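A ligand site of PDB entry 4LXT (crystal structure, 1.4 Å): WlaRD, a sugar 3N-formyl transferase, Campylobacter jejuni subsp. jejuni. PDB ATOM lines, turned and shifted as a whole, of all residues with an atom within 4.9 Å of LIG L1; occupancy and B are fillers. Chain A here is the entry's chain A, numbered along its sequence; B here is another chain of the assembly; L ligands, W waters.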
ATOM      1  N   SER A  77      28.522  -0.772  15.026  1.00  0.00           N
ATOM      2  CA  SER A  77      28.908  -1.937  15.844  1.00  0.00           C
ATOM      3  C   SER A  77      29.898  -2.823  15.113  1.00  0.00           C
ATOM      4  O   SER A  77      29.671  -3.220  13.973  1.00  0.00           O
ATOM      5  CB  SER A  77      27.664  -2.776  16.062  1.00  0.00           C
ATOM      6  OG  SER A  77      27.990  -4.079  16.540  1.00  0.00           O
ATOM      7  N   PHE A  80      30.267  -5.614  18.873  1.00  0.00           N
ATOM      8  CA  PHE A  80      29.666  -5.064  20.091  1.00  0.00           C
ATOM      9  C   PHE A  80      28.838  -6.099  20.846  1.00  0.00           C
ATOM     10  O   PHE A  80      28.169  -6.955  20.229  1.00  0.00           O
ATOM     11  CB  PHE A  80      28.785  -3.868  19.681  1.00  0.00           C
ATOM     12  CG  PHE A  80      28.284  -3.016  20.780  1.00  0.00           C
ATOM     13  CD1 PHE A  80      26.944  -2.600  20.752  1.00  0.00           C
ATOM     14  CD2 PHE A  80      29.111  -2.595  21.815  1.00  0.00           C
ATOM     15  CE1 PHE A  80      26.452  -1.747  21.736  1.00  0.00           C
ATOM     16  CE2 PHE A  80      28.619  -1.786  22.831  1.00  0.00           C
ATOM     17  CZ  PHE A  80      27.293  -1.342  22.765  1.00  0.00           C
ATOM     18  N   ASP A  81      28.862  -5.985  22.165  1.00  0.00           N
ATOM     19  CA  ASP A  81      28.306  -7.002  23.051  1.00  0.00           C
ATOM     20  C   ASP A  81      26.869  -6.744  23.472  1.00  0.00           C
ATOM     21  O   ASP A  81      26.294  -7.573  24.194  1.00  0.00           O
ATOM     22  CB  ASP A  81      29.193  -7.264  24.282  1.00  0.00           C
ATOM     23  CG  ASP A  81      29.381  -6.040  25.145  1.00  0.00           C
ATOM     24  OD1 ASP A  81      29.947  -6.193  26.264  1.00  0.00           O
ATOM     25  OD2 ASP A  81      29.002  -4.905  24.783  1.00  0.00           O
ATOM     26  N   GLN A  82      26.294  -5.600  23.105  1.00  0.00           N
ATOM     27  CA  GLN A  82      24.924  -5.265  23.534  1.00  0.00           C
ATOM     28  C   GLN A  82      23.960  -5.252  22.375  1.00  0.00           C
ATOM     29  O   GLN A  82      24.269  -4.718  21.323  1.00  0.00           O
ATOM     30  CB  GLN A  82      24.819  -3.894  24.223  1.00  0.00           C
ATOM     31  CG  GLN A  82      25.716  -3.782  25.462  1.00  0.00           C
ATOM     32  CD  GLN A  82      25.504  -2.472  26.187  1.00  0.00           C
ATOM     33  OE1 GLN A  82      24.388  -2.268  26.697  1.00  0.00           O
ATOM     34  NE2 GLN A  82      26.500  -1.595  26.263  1.00  0.00           N
ATOM     35  N   ILE A  83      22.785  -5.847  22.563  1.00  0.00           N
ATOM     36  CA  ILE A  83      21.699  -5.787  21.580  1.00  0.00           C
ATOM     37  C   ILE A  83      20.949  -4.466  21.801  1.00  0.00           C
ATOM     38  O   ILE A  83      20.507  -4.181  22.861  1.00  0.00           O
ATOM     39  CB  ILE A  83      20.735  -6.968  21.729  1.00  0.00           C
ATOM     40  CG1 ILE A  83      21.494  -8.273  21.476  1.00  0.00           C
ATOM     41  CG2 ILE A  83      19.544  -6.831  20.733  1.00  0.00           C
ATOM     42  CD1 ILE A  83      20.759  -9.510  22.059  1.00  0.00           C
ATOM     43  N   ILE A  84      20.964  -3.652  20.771  1.00  0.00           N
ATOM     44  CA  ILE A  84      20.339  -2.315  20.896  1.00  0.00           C
ATOM     45  C   ILE A  84      18.879  -2.390  20.488  1.00  0.00           C
ATOM     46  O   ILE A  84      18.433  -3.331  19.785  1.00  0.00           O
ATOM     47  CB  ILE A  84      21.108  -1.241  20.090  1.00  0.00           C
ATOM     48  CG1 ILE A  84      21.015  -1.444  18.586  1.00  0.00           C
ATOM     49  CG2 ILE A  84      22.586  -1.079  20.592  1.00  0.00           C
ATOM     50  CD1 ILE A  84      21.370  -0.175  17.767  1.00  0.00           C
ATOM     51  N   ASN A  96      26.094  -2.545  11.392  1.00  0.00           N
ATOM     52  CA  ASN A  96      26.889  -3.621  12.052  1.00  0.00           C
ATOM     53  C   ASN A  96      27.588  -4.388  10.954  1.00  0.00           C
ATOM     54  O   ASN A  96      27.128  -4.491   9.821  1.00  0.00           O
ATOM     55  CB  ASN A  96      25.925  -4.572  12.744  1.00  0.00           C
ATOM     56  CG  ASN A  96      26.638  -5.746  13.412  1.00  0.00           C
ATOM     57  OD1 ASN A  96      26.401  -6.926  13.023  1.00  0.00           O
ATOM     58  ND2 ASN A  96      27.441  -5.462  14.383  1.00  0.00           N
ATOM     59  N   HIS A  98      28.567  -8.267  10.667  1.00  0.00           N
ATOM     60  CA  HIS A  98      28.341  -9.589  11.260  1.00  0.00           C
ATOM     61  C   HIS A  98      29.261 -10.595  10.610  1.00  0.00           C
ATOM     62  O   HIS A  98      29.396 -10.632   9.398  1.00  0.00           O
ATOM     63  CB  HIS A  98      26.871 -10.031  11.084  1.00  0.00           C
ATOM     64  CG  HIS A  98      26.616 -11.366  11.720  1.00  0.00           C
ATOM     65  ND1 HIS A  98      26.605 -11.540  13.087  1.00  0.00           N
ATOM     66  CD2 HIS A  98      26.373 -12.579  11.181  1.00  0.00           C
ATOM     67  CE1 HIS A  98      26.359 -12.817  13.353  1.00  0.00           C
ATOM     68  NE2 HIS A  98      26.229 -13.467  12.219  1.00  0.00           N
ATOM     69  N   GLY A 107      23.357 -14.922  15.159  1.00  0.00           N
ATOM     70  CA  GLY A 107      23.556 -15.258  16.572  1.00  0.00           C
ATOM     71  C   GLY A 107      25.031 -15.210  16.922  1.00  0.00           C
ATOM     72  O   GLY A 107      25.692 -14.206  16.616  1.00  0.00           O
ATOM     73  N   VAL A 108      25.519 -16.220  17.634  1.00  0.00           N
ATOM     74  CA  VAL A 108      26.838 -16.166  18.294  1.00  0.00           C
ATOM     75  C   VAL A 108      27.692 -17.348  17.827  1.00  0.00           C
ATOM     76  O   VAL A 108      27.248 -18.224  17.066  1.00  0.00           O
ATOM     77  CB  VAL A 108      26.720 -16.105  19.825  1.00  0.00           C
ATOM     78  CG1 VAL A 108      25.857 -14.870  20.216  1.00  0.00           C
ATOM     79  CG2 VAL A 108      26.105 -17.384  20.319  1.00  0.00           C
ATOM     80  N   HIS A 127      25.444  -4.764   7.432  1.00  0.00           N
ATOM     81  CA  HIS A 127      23.966  -4.636   7.385  1.00  0.00           C
ATOM     82  C   HIS A 127      23.478  -3.513   8.292  1.00  0.00           C
ATOM     83  O   HIS A 127      24.155  -3.070   9.219  1.00  0.00           O
ATOM     84  CB  HIS A 127      23.296  -5.979   7.752  1.00  0.00           C
ATOM     85  CG  HIS A 127      23.555  -6.442   9.156  1.00  0.00           C
ATOM     86  ND1 HIS A 127      22.728  -6.152  10.209  1.00  0.00           N
ATOM     87  CD2 HIS A 127      24.578  -7.162   9.701  1.00  0.00           C
ATOM     88  CE1 HIS A 127      23.185  -6.656  11.351  1.00  0.00           C
ATOM     89  NE2 HIS A 127      24.305  -7.292  11.039  1.00  0.00           N
ATOM     90  N   ILE A 129      21.294  -2.260  11.398  1.00  0.00           N
ATOM     91  CA  ILE A 129      20.783  -2.854  12.611  1.00  0.00           C
ATOM     92  C   ILE A 129      19.297  -2.596  12.665  1.00  0.00           C
ATOM     93  O   ILE A 129      18.840  -1.425  12.588  1.00  0.00           O
ATOM     94  CB  ILE A 129      21.455  -2.272  13.865  1.00  0.00           C
ATOM     95  CG1 ILE A 129      22.944  -2.630  13.822  1.00  0.00           C
ATOM     96  CG2 ILE A 129      20.806  -2.766  15.155  1.00  0.00           C
ATOM     97  CD1 ILE A 129      23.727  -1.971  14.941  1.00  0.00           C
ATOM     98  N   ASP A 130      18.502  -3.649  12.836  1.00  0.00           N
ATOM     99  CA  ASP A 130      17.099  -3.556  13.266  1.00  0.00           C
ATOM    100  C   ASP A 130      16.926  -4.197  14.624  1.00  0.00           C
ATOM    101  O   ASP A 130      17.952  -4.563  15.261  1.00  0.00           O
ATOM    102  CB  ASP A 130      16.137  -4.058  12.193  1.00  0.00           C
ATOM    103  CG  ASP A 130      16.248  -5.564  11.955  1.00  0.00           C
ATOM    104  OD1 ASP A 130      15.701  -5.988  10.906  1.00  0.00           O
ATOM    105  OD2 ASP A 130      16.856  -6.275  12.800  1.00  0.00           O
ATOM    106  N   ASN A 131      15.731  -4.366  15.169  1.00  0.00           N
ATOM    107  CA  ASN A 131      15.598  -4.832  16.520  1.00  0.00           C
ATOM    108  C   ASN A 131      15.907  -6.335  16.738  1.00  0.00           C
ATOM    109  O   ASN A 131      16.051  -6.745  17.877  1.00  0.00           O
ATOM    110  CB  ASN A 131      14.200  -4.533  17.055  1.00  0.00           C
ATOM    111  CG  ASN A 131      14.110  -3.085  17.567  1.00  0.00           C
ATOM    112  OD1 ASN A 131      15.084  -2.457  17.980  1.00  0.00           O
ATOM    113  ND2 ASN A 131      12.897  -2.548  17.448  1.00  0.00           N
ATOM    114  N   GLY A 132      15.962  -7.067  15.634  1.00  0.00           N
ATOM    115  CA  GLY A 132      16.344  -8.484  15.768  1.00  0.00           C
ATOM    116  C   GLY A 132      17.856  -8.682  15.726  1.00  0.00           C
ATOM    117  O   GLY A 132      18.641  -7.789  15.382  1.00  0.00           O
ATOM    118  N   ILE A 133      18.231  -9.930  15.980  1.00  0.00           N
ATOM    119  CA  ILE A 133      19.657 -10.327  16.029  1.00  0.00           C
ATOM    120  C   ILE A 133      20.119 -10.692  14.600  1.00  0.00           C
ATOM    121  O   ILE A 133      19.732 -11.732  14.036  1.00  0.00           O
ATOM    122  CB  ILE A 133      19.862 -11.458  17.025  1.00  0.00           C
ATOM    123  CG1 ILE A 133      19.499 -11.016  18.446  1.00  0.00           C
ATOM    124  CG2 ILE A 133      21.388 -11.812  16.982  1.00  0.00           C
ATOM    125  CD1 ILE A 133      19.491 -12.162  19.468  1.00  0.00           C
ATOM    126  N   ASP A 134      20.919  -9.831  13.987  1.00  0.00           N
ATOM    127  CA  ASP A 134      21.480 -10.003  12.667  1.00  0.00           C
ATOM    128  C   ASP A 134      20.482 -10.130  11.528  1.00  0.00           C
ATOM    129  O   ASP A 134      20.753 -10.764  10.508  1.00  0.00           O
ATOM    130  CB  ASP A 134      22.437 -11.226  12.645  1.00  0.00           C
ATOM    131  CG  ASP A 134      23.431 -11.195  13.801  1.00  0.00           C
ATOM    132  OD1 ASP A 134      24.007 -10.114  14.083  1.00  0.00           O
ATOM    133  OD2 ASP A 134      23.661 -12.244  14.441  1.00  0.00           O
ATOM    134  N   THR A 135      19.344  -9.443  11.711  1.00  0.00           N
ATOM    135  CA  THR A 135      18.193  -9.581  10.837  1.00  0.00           C
ATOM    136  C   THR A 135      18.021  -8.420   9.866  1.00  0.00           C
ATOM    137  O   THR A 135      17.239  -8.545   8.911  1.00  0.00           O
ATOM    138  CB  THR A 135      16.916  -9.744  11.715  1.00  0.00           C
ATOM    139  OG1 THR A 135      16.973  -8.824  12.807  1.00  0.00           O
ATOM    140  CG2 THR A 135      16.807 -11.178  12.341  1.00  0.00           C
ATOM    141  N   TYR A 191      20.290 -19.629  12.864  1.00  0.00           N
ATOM    142  CA  TYR A 191      20.553 -18.860  14.069  1.00  0.00           C
ATOM    143  C   TYR A 191      21.022 -19.807  15.148  1.00  0.00           C
ATOM    144  O   TYR A 191      20.454 -20.871  15.322  1.00  0.00           O
ATOM    145  CB  TYR A 191      19.318 -18.097  14.568  1.00  0.00           C
ATOM    146  CG  TYR A 191      19.405 -17.505  15.963  1.00  0.00           C
ATOM    147  CD1 TYR A 191      19.963 -16.238  16.175  1.00  0.00           C
ATOM    148  CD2 TYR A 191      18.930 -18.185  17.087  1.00  0.00           C
ATOM    149  CE1 TYR A 191      20.040 -15.673  17.412  1.00  0.00           C
ATOM    150  CE2 TYR A 191      19.006 -17.639  18.336  1.00  0.00           C
ATOM    151  CZ  TYR A 191      19.546 -16.364  18.494  1.00  0.00           C
ATOM    152  OH  TYR A 191      19.610 -15.801  19.735  1.00  0.00           O
ATOM    153  N   PHE A 192      22.092 -19.423  15.852  1.00  0.00           N
ATOM    154  CA  PHE A 192      22.596 -20.245  16.953  1.00  0.00           C
ATOM    155  C   PHE A 192      22.783 -19.345  18.164  1.00  0.00           C
ATOM    156  O   PHE A 192      23.434 -18.290  18.058  1.00  0.00           O
ATOM    157  CB  PHE A 192      23.907 -20.961  16.599  1.00  0.00           C
ATOM    158  CG  PHE A 192      23.704 -21.961  15.503  1.00  0.00           C
ATOM    159  CD1 PHE A 192      23.397 -23.287  15.796  1.00  0.00           C
ATOM    160  CD2 PHE A 192      23.699 -21.554  14.190  1.00  0.00           C
ATOM    161  CE1 PHE A 192      23.131 -24.196  14.777  1.00  0.00           C
ATOM    162  CE2 PHE A 192      23.416 -22.459  13.169  1.00  0.00           C
ATOM    163  CZ  PHE A 192      23.153 -23.794  13.476  1.00  0.00           C
ATOM    164  N   SER A 193      22.285 -19.745  19.316  1.00  0.00           N
ATOM    165  CA  SER A 193      22.488 -19.044  20.558  1.00  0.00           C
ATOM    166  C   SER A 193      23.518 -19.729  21.421  1.00  0.00           C
ATOM    167  O   SER A 193      23.920 -20.850  21.092  1.00  0.00           O
ATOM    168  CB  SER A 193      21.187 -18.778  21.313  1.00  0.00           C
ATOM    169  OG  SER A 193      20.669 -20.017  21.731  1.00  0.00           O
ATOM    170  N   ARG A 194      23.925 -19.104  22.523  1.00  0.00           N
ATOM    171  CA  ARG A 194      24.940 -19.718  23.369  1.00  0.00           C
ATOM    172  C   ARG A 194      24.482 -21.107  23.841  1.00  0.00           C
ATOM    173  O   ARG A 194      25.313 -22.023  23.887  1.00  0.00           O
ATOM    174  CB  ARG A 194      25.232 -18.867  24.604  1.00  0.00           C
ATOM    175  CG  ARG A 194      26.001 -17.593  24.286  1.00  0.00           C
ATOM    176  CD  ARG A 194      26.466 -16.760  25.541  1.00  0.00           C
ATOM    177  NE  ARG A 194      26.933 -15.470  25.009  1.00  0.00           N
ATOM    178  CZ  ARG A 194      26.210 -14.357  24.986  1.00  0.00           C
ATOM    179  NH1 ARG A 194      25.009 -14.278  25.552  1.00  0.00           N
ATOM    180  NH2 ARG A 194      26.743 -13.286  24.378  1.00  0.00           N
ATOM    181  N   LYS A 195      23.215 -21.297  24.150  1.00  0.00           N
ATOM    182  CA  LYS A 195      22.743 -22.564  24.676  1.00  0.00           C
ATOM    183  C   LYS A 195      22.838 -23.651  23.611  1.00  0.00           C
ATOM    184  O   LYS A 195      22.779 -24.837  23.942  1.00  0.00           O
ATOM    185  CB  LYS A 195      21.285 -22.441  25.157  1.00  0.00           C
ATOM    186  CG  LYS A 195      20.273 -22.616  24.024  1.00  0.00           C
ATOM    187  CD  LYS A 195      18.848 -22.471  24.550  1.00  0.00           C
ATOM    188  CE  LYS A 195      18.000 -21.889  23.437  1.00  0.00           C
ATOM    189  NZ  LYS A 195      17.768 -22.954  22.437  1.00  0.00           N
ATOM    190  N   LYS B 206      13.933 -20.900  19.787  1.00  0.00           N
ATOM    191  CA  LYS B 206      14.938 -19.828  19.721  1.00  0.00           C
ATOM    192  C   LYS B 206      15.775 -20.058  18.466  1.00  0.00           C
ATOM    193  O   LYS B 206      16.988 -20.328  18.535  1.00  0.00           O
ATOM    194  CB  LYS B 206      15.790 -19.800  20.992  1.00  0.00           C
ATOM    195  CG  LYS B 206      15.020 -19.356  22.220  1.00  0.00           C
ATOM    196  CD  LYS B 206      14.586 -17.909  22.079  1.00  0.00           C
ATOM    197  CE  LYS B 206      14.302 -17.236  23.427  1.00  0.00           C
ATOM    198  NZ  LYS B 206      14.251 -18.246  24.514  1.00  0.00           N
HETATM  199  N1  LIG L   1      21.690  -4.975  18.204  1.00  0.00           N
HETATM  200  C1  LIG L   1      20.660  -5.358  17.414  1.00  0.00           C
HETATM  201  N2  LIG L   1      19.394  -4.934  17.693  1.00  0.00           N
HETATM  202  N3  LIG L   1      20.787  -6.112  16.314  1.00  0.00           N
HETATM  203  C2  LIG L   1      21.975  -6.626  15.965  1.00  0.00           C
HETATM  204  O1  LIG L   1      21.976  -7.314  14.825  1.00  0.00           O
HETATM  205  C3  LIG L   1      23.103  -6.292  16.712  1.00  0.00           C
HETATM  206  N4  LIG L   1      24.382  -6.894  16.538  1.00  0.00           N
HETATM  207  C4  LIG L   1      25.313  -6.824  17.700  1.00  0.00           C
HETATM  208  C5  LIG L   1      25.299  -5.385  18.212  1.00  0.00           C
HETATM  209  N5  LIG L   1      23.908  -5.105  18.645  1.00  0.00           N
HETATM  210  C6  LIG L   1      22.883  -5.504  17.839  1.00  0.00           C
HETATM  211  C7  LIG L   1      25.003  -7.584  19.002  1.00  0.00           C
HETATM  212  N6  LIG L   1      25.320  -8.996  18.934  1.00  0.00           N
HETATM  213  C8  LIG L   1      23.936 -11.598  21.908  1.00  0.00           C
HETATM  214  C9  LIG L   1      24.556 -10.383  22.242  1.00  0.00           C
HETATM  215  C10 LIG L   1      25.034  -9.514  21.236  1.00  0.00           C
HETATM  216  C11 LIG L   1      24.878  -9.817  19.910  1.00  0.00           C
HETATM  217  C12 LIG L   1      24.259 -11.013  19.563  1.00  0.00           C
HETATM  218  C13 LIG L   1      23.795 -11.861  20.554  1.00  0.00           C
HETATM  219  C14 LIG L   1      23.406 -12.458  23.013  1.00  0.00           C
HETATM  220  O2  LIG L   1      23.523 -12.151  24.193  1.00  0.00           O
HETATM  221  N7  LIG L   1      22.701 -13.544  22.632  1.00  0.00           N
HETATM  222  C15 LIG L   1      22.054 -14.438  23.594  1.00  0.00           C
HETATM  223  C16 LIG L   1      20.552 -14.455  23.198  1.00  0.00           C
HETATM  224  C17 LIG L   1      19.860 -13.123  23.556  1.00  0.00           C
HETATM  225  C18 LIG L   1      18.359 -13.138  23.328  1.00  0.00           C
HETATM  226  O3  LIG L   1      17.756 -14.202  23.087  1.00  0.00           O
HETATM  227  O4  LIG L   1      17.777 -12.017  23.445  1.00  0.00           O
HETATM  228  C19 LIG L   1      22.561 -15.872  23.549  1.00  0.00           C
HETATM  229  O5  LIG L   1      23.051 -16.303  22.482  1.00  0.00           O
HETATM  230  O6  LIG L   1      22.421 -16.549  24.597  1.00  0.00           O
HETATM  231  C20 LIG L   1      24.705  -7.668  15.571  1.00  0.00           C
HETATM  232  O7  LIG L   1      25.801  -8.286  15.547  1.00  0.00           O
HETATM  233  O1  LG2 L   2      34.526 -19.616  25.032  1.00  0.00           O
HETATM  234  C1  LG2 L   2      34.683 -19.335  23.818  1.00  0.00           C
HETATM  235  N1  LG2 L   2      35.171 -20.277  22.968  1.00  0.00           N
HETATM  236  C2  LG2 L   2      35.412 -20.031  21.673  1.00  0.00           C
HETATM  237  O2  LG2 L   2      35.858 -20.902  20.888  1.00  0.00           O
HETATM  238  C3  LG2 L   2      34.401 -18.055  23.260  1.00  0.00           C
HETATM  239  C4  LG2 L   2      33.852 -16.957  24.173  1.00  0.00           C
HETATM  240  C5  LG2 L   2      34.635 -17.871  21.985  1.00  0.00           C
HETATM  241  N2  LG2 L   2      35.118 -18.796  21.151  1.00  0.00           N
HETATM  242  C6  LG2 L   2      35.398 -18.543  19.748  1.00  0.00           C
HETATM  243  O3  LG2 L   2      35.844 -17.204  19.545  1.00  0.00           O
HETATM  244  C7  LG2 L   2      34.282 -18.807  18.765  1.00  0.00           C
HETATM  245  C8  LG2 L   2      33.722 -17.398  18.564  1.00  0.00           C
HETATM  246  O4  LG2 L   2      33.020 -17.371  17.315  1.00  0.00           O
HETATM  247  C9  LG2 L   2      34.968 -16.572  18.555  1.00  0.00           C
HETATM  248  C10 LG2 L   2      34.746 -15.131  18.980  1.00  0.00           C
HETATM  249  O5  LG2 L   2      34.056 -15.151  20.208  1.00  0.00           O
HETATM  250  P1  LG2 L   2      33.355 -13.791  20.691  1.00  0.00           P
HETATM  251  O6  LG2 L   2      34.267 -12.613  20.450  1.00  0.00           O
HETATM  252  O7  LG2 L   2      32.871 -14.037  22.023  1.00  0.00           O
HETATM  253  O8  LG2 L   2      32.145 -13.550  19.681  1.00  0.00           O
HETATM  254  P2  LG2 L   2      31.099 -14.426  18.838  1.00  0.00           P
HETATM  255  O9  LG2 L   2      30.335 -15.294  19.749  1.00  0.00           O
HETATM  256  O10 LG2 L   2      31.718 -14.978  17.654  1.00  0.00           O
HETATM  257  O11 LG2 L   2      30.138 -13.233  18.295  1.00  0.00           O
HETATM  258  O12 LG2 L   2      29.203  -8.721  18.410  1.00  0.00           O
HETATM  259  C11 LG2 L   2      28.793 -10.063  18.816  1.00  0.00           C
HETATM  260  C12 LG2 L   2      29.838 -10.771  19.694  1.00  0.00           C
HETATM  261  O13 LG2 L   2      29.189 -12.016  20.026  1.00  0.00           O
HETATM  262  C13 LG2 L   2      30.179 -10.104  21.027  1.00  0.00           C
HETATM  263  C14 LG2 L   2      28.694 -10.810  17.503  1.00  0.00           C
HETATM  264  N3  LG2 L   2      27.850 -10.115  16.498  1.00  0.00           N
HETATM  265  C15 LG2 L   2      28.087 -12.196  17.834  1.00  0.00           C
HETATM  266  O14 LG2 L   2      28.099 -12.960  16.651  1.00  0.00           O
HETATM  267  C16 LG2 L   2      28.928 -12.851  18.916  1.00  0.00           C
HETATM  268  O   HOH W   1      23.441 -15.790  27.180  1.00  0.00           O
HETATM  269  O   HOH W   2      19.747  -6.463  12.953  1.00  0.00           O
HETATM  270  O   HOH W   3      18.921 -10.068  25.297  1.00  0.00           O
HETATM  271  O   HOH W   4      25.278 -11.217  16.409  1.00  0.00           O
HETATM  272  O   HOH W   5      18.234 -16.823  21.780  1.00  0.00           O
HETATM  273  O   HOH W   6      22.335 -14.978  20.115  1.00  0.00           O
HETATM  274  O   HOH W   7      16.916  -9.502  21.658  1.00  0.00           O
HETATM  275  O   HOH W   8      18.757 -13.884  26.757  1.00  0.00           O
HETATM  276  O   HOH W   9      29.216  -7.637  15.339  1.00  0.00           O
HETATM  277  O   HOH W  10      20.895 -15.647  26.658  1.00  0.00           O
HETATM  278  O   HOH W  11      22.383 -10.135  25.510  1.00  0.00           O
HETATM  279  O   HOH W  12      21.482 -19.032  24.915  1.00  0.00           O
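OG of Ser 77 touches C5 of LIG L1, at 3.4 Å.
O of Phe 80 touches C7 of LIG L1, 3.5 Å away.
Asp 81 touches LIG L1.
CA of Ile 83 touches N1 of LIG L1, 3.5 Å away.
CG1 of Val 108 touches C13 of LIG L1, 3.7 Å away.
CE1 of His 127 touches O1 of LIG L1, 3.7 Å away.
Ile 129 touches LIG L1.
Asn 131 touches LIG L1 (O to N2, 3.8 Å).
Ile 133 touches LIG L1.
Tyr 191 touches LIG L1.
Ser 193 touches LIG L1.
The nearest printed residue that does not touch LIG L1 is His 98 (4.2 Å).
O5 of LIG L1 sits at hydrogen-bond distance from N of Arg 194 (2.9 Å).
N3 of LIG L1 lies close to O of Gly 132, at 2.9 Å.
The backbone carbonyl oxygen (O) of Ile 84 is in hydrogen-bond range of a nitrogen (N2) of LIG L1 (2.8 Å).
The guanidinium group (NH1) of Arg 194 lies within salt-bridge range of an oxygen (O6) of LIG L1, at 3.6 Å.
A nitrogen (N1) of LIG L1 is in hydrogen-bond range of the backbone NH (N) of Ile 84 (3.0 Å).
N of Phe 80 lies within hydrogen-bond range of O12 of LG2 L2 (3.3 Å).
O14 of LG2 L2 is in hydrogen-bond range of O of Gly 107 (2.7 Å).
O of Asp 130 lies within hydrogen-bond range of N2 of LIG L1 (2.9 Å).
OD1 of Asn 96 lies close to O7 of LIG L1, 2.9 Å away.
O of Gln 82 sits at hydrogen-bond distance from N5 of LIG L1, at 2.7 Å.
An oxygen (O12) of LG2 L2 sits at hydrogen-bond distance from the backbone carbonyl oxygen of Phe 80 (2.7 Å).
O1 of LIG L1 lies within hydrogen-bond range of N of Asp 134 (2.9 Å).
Water W12 lies within hydrogen-bond range of O6 of LIG L1, N of Lys 195, N of Arg 194 and OG of Ser 193.
Water W6 lies within hydrogen-bond range of O5 of LIG L1 (2.8 Å) and OH of Tyr 191 (2.9 Å).
Water W1 bridges NH1 of Arg 194 (2.7 Å) and O6 of LIG L1 (2.9 Å).
Water W5 lies within hydrogen-bond range of the side-chain hydroxyl of Tyr 191 (2.7 Å) and an oxygen (O3) of LIG L1 (3.0 Å).
Water W9 lies within hydrogen-bond range of ND2 of Asn 96 (3.0 Å), N3 of LG2 L2 (3.1 Å) and O7 of LIG L1 (3.5 Å).
N3 of LG2 L2 is in hydrogen-bond range of O7 of LIG L1, at 2.9 Å.
The side-chain amide nitrogen of Asn 96 sits at hydrogen-bond distance from the side-chain hydroxyl of Ser 77 (2.6 Å).
OG1 of Thr 135 lies within hydrogen-bond range of OD2 of Asp 130, at 2.6 Å.
ND1 of His 98 sits at hydrogen-bond distance from OD1 of Asp 134 (3.1 Å).
O of Phe 192 sits at hydrogen-bond distance from N of Val 108 (3.0 Å).
O of Gly 132 lies close to OG1 of Thr 135 (3.2 Å).
A ring nitrogen (NE2) of His 127 is in hydrogen-bond range of the side-chain amide oxygen (OD1) of Asn 96 (2.9 Å).
OD2 of Asp 130 sits at hydrogen-bond distance from N of Gly 132 (3.1 Å).
OD2 of Asp 134 sits at hydrogen-bond distance from N of Gly 107 (2.8 Å).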
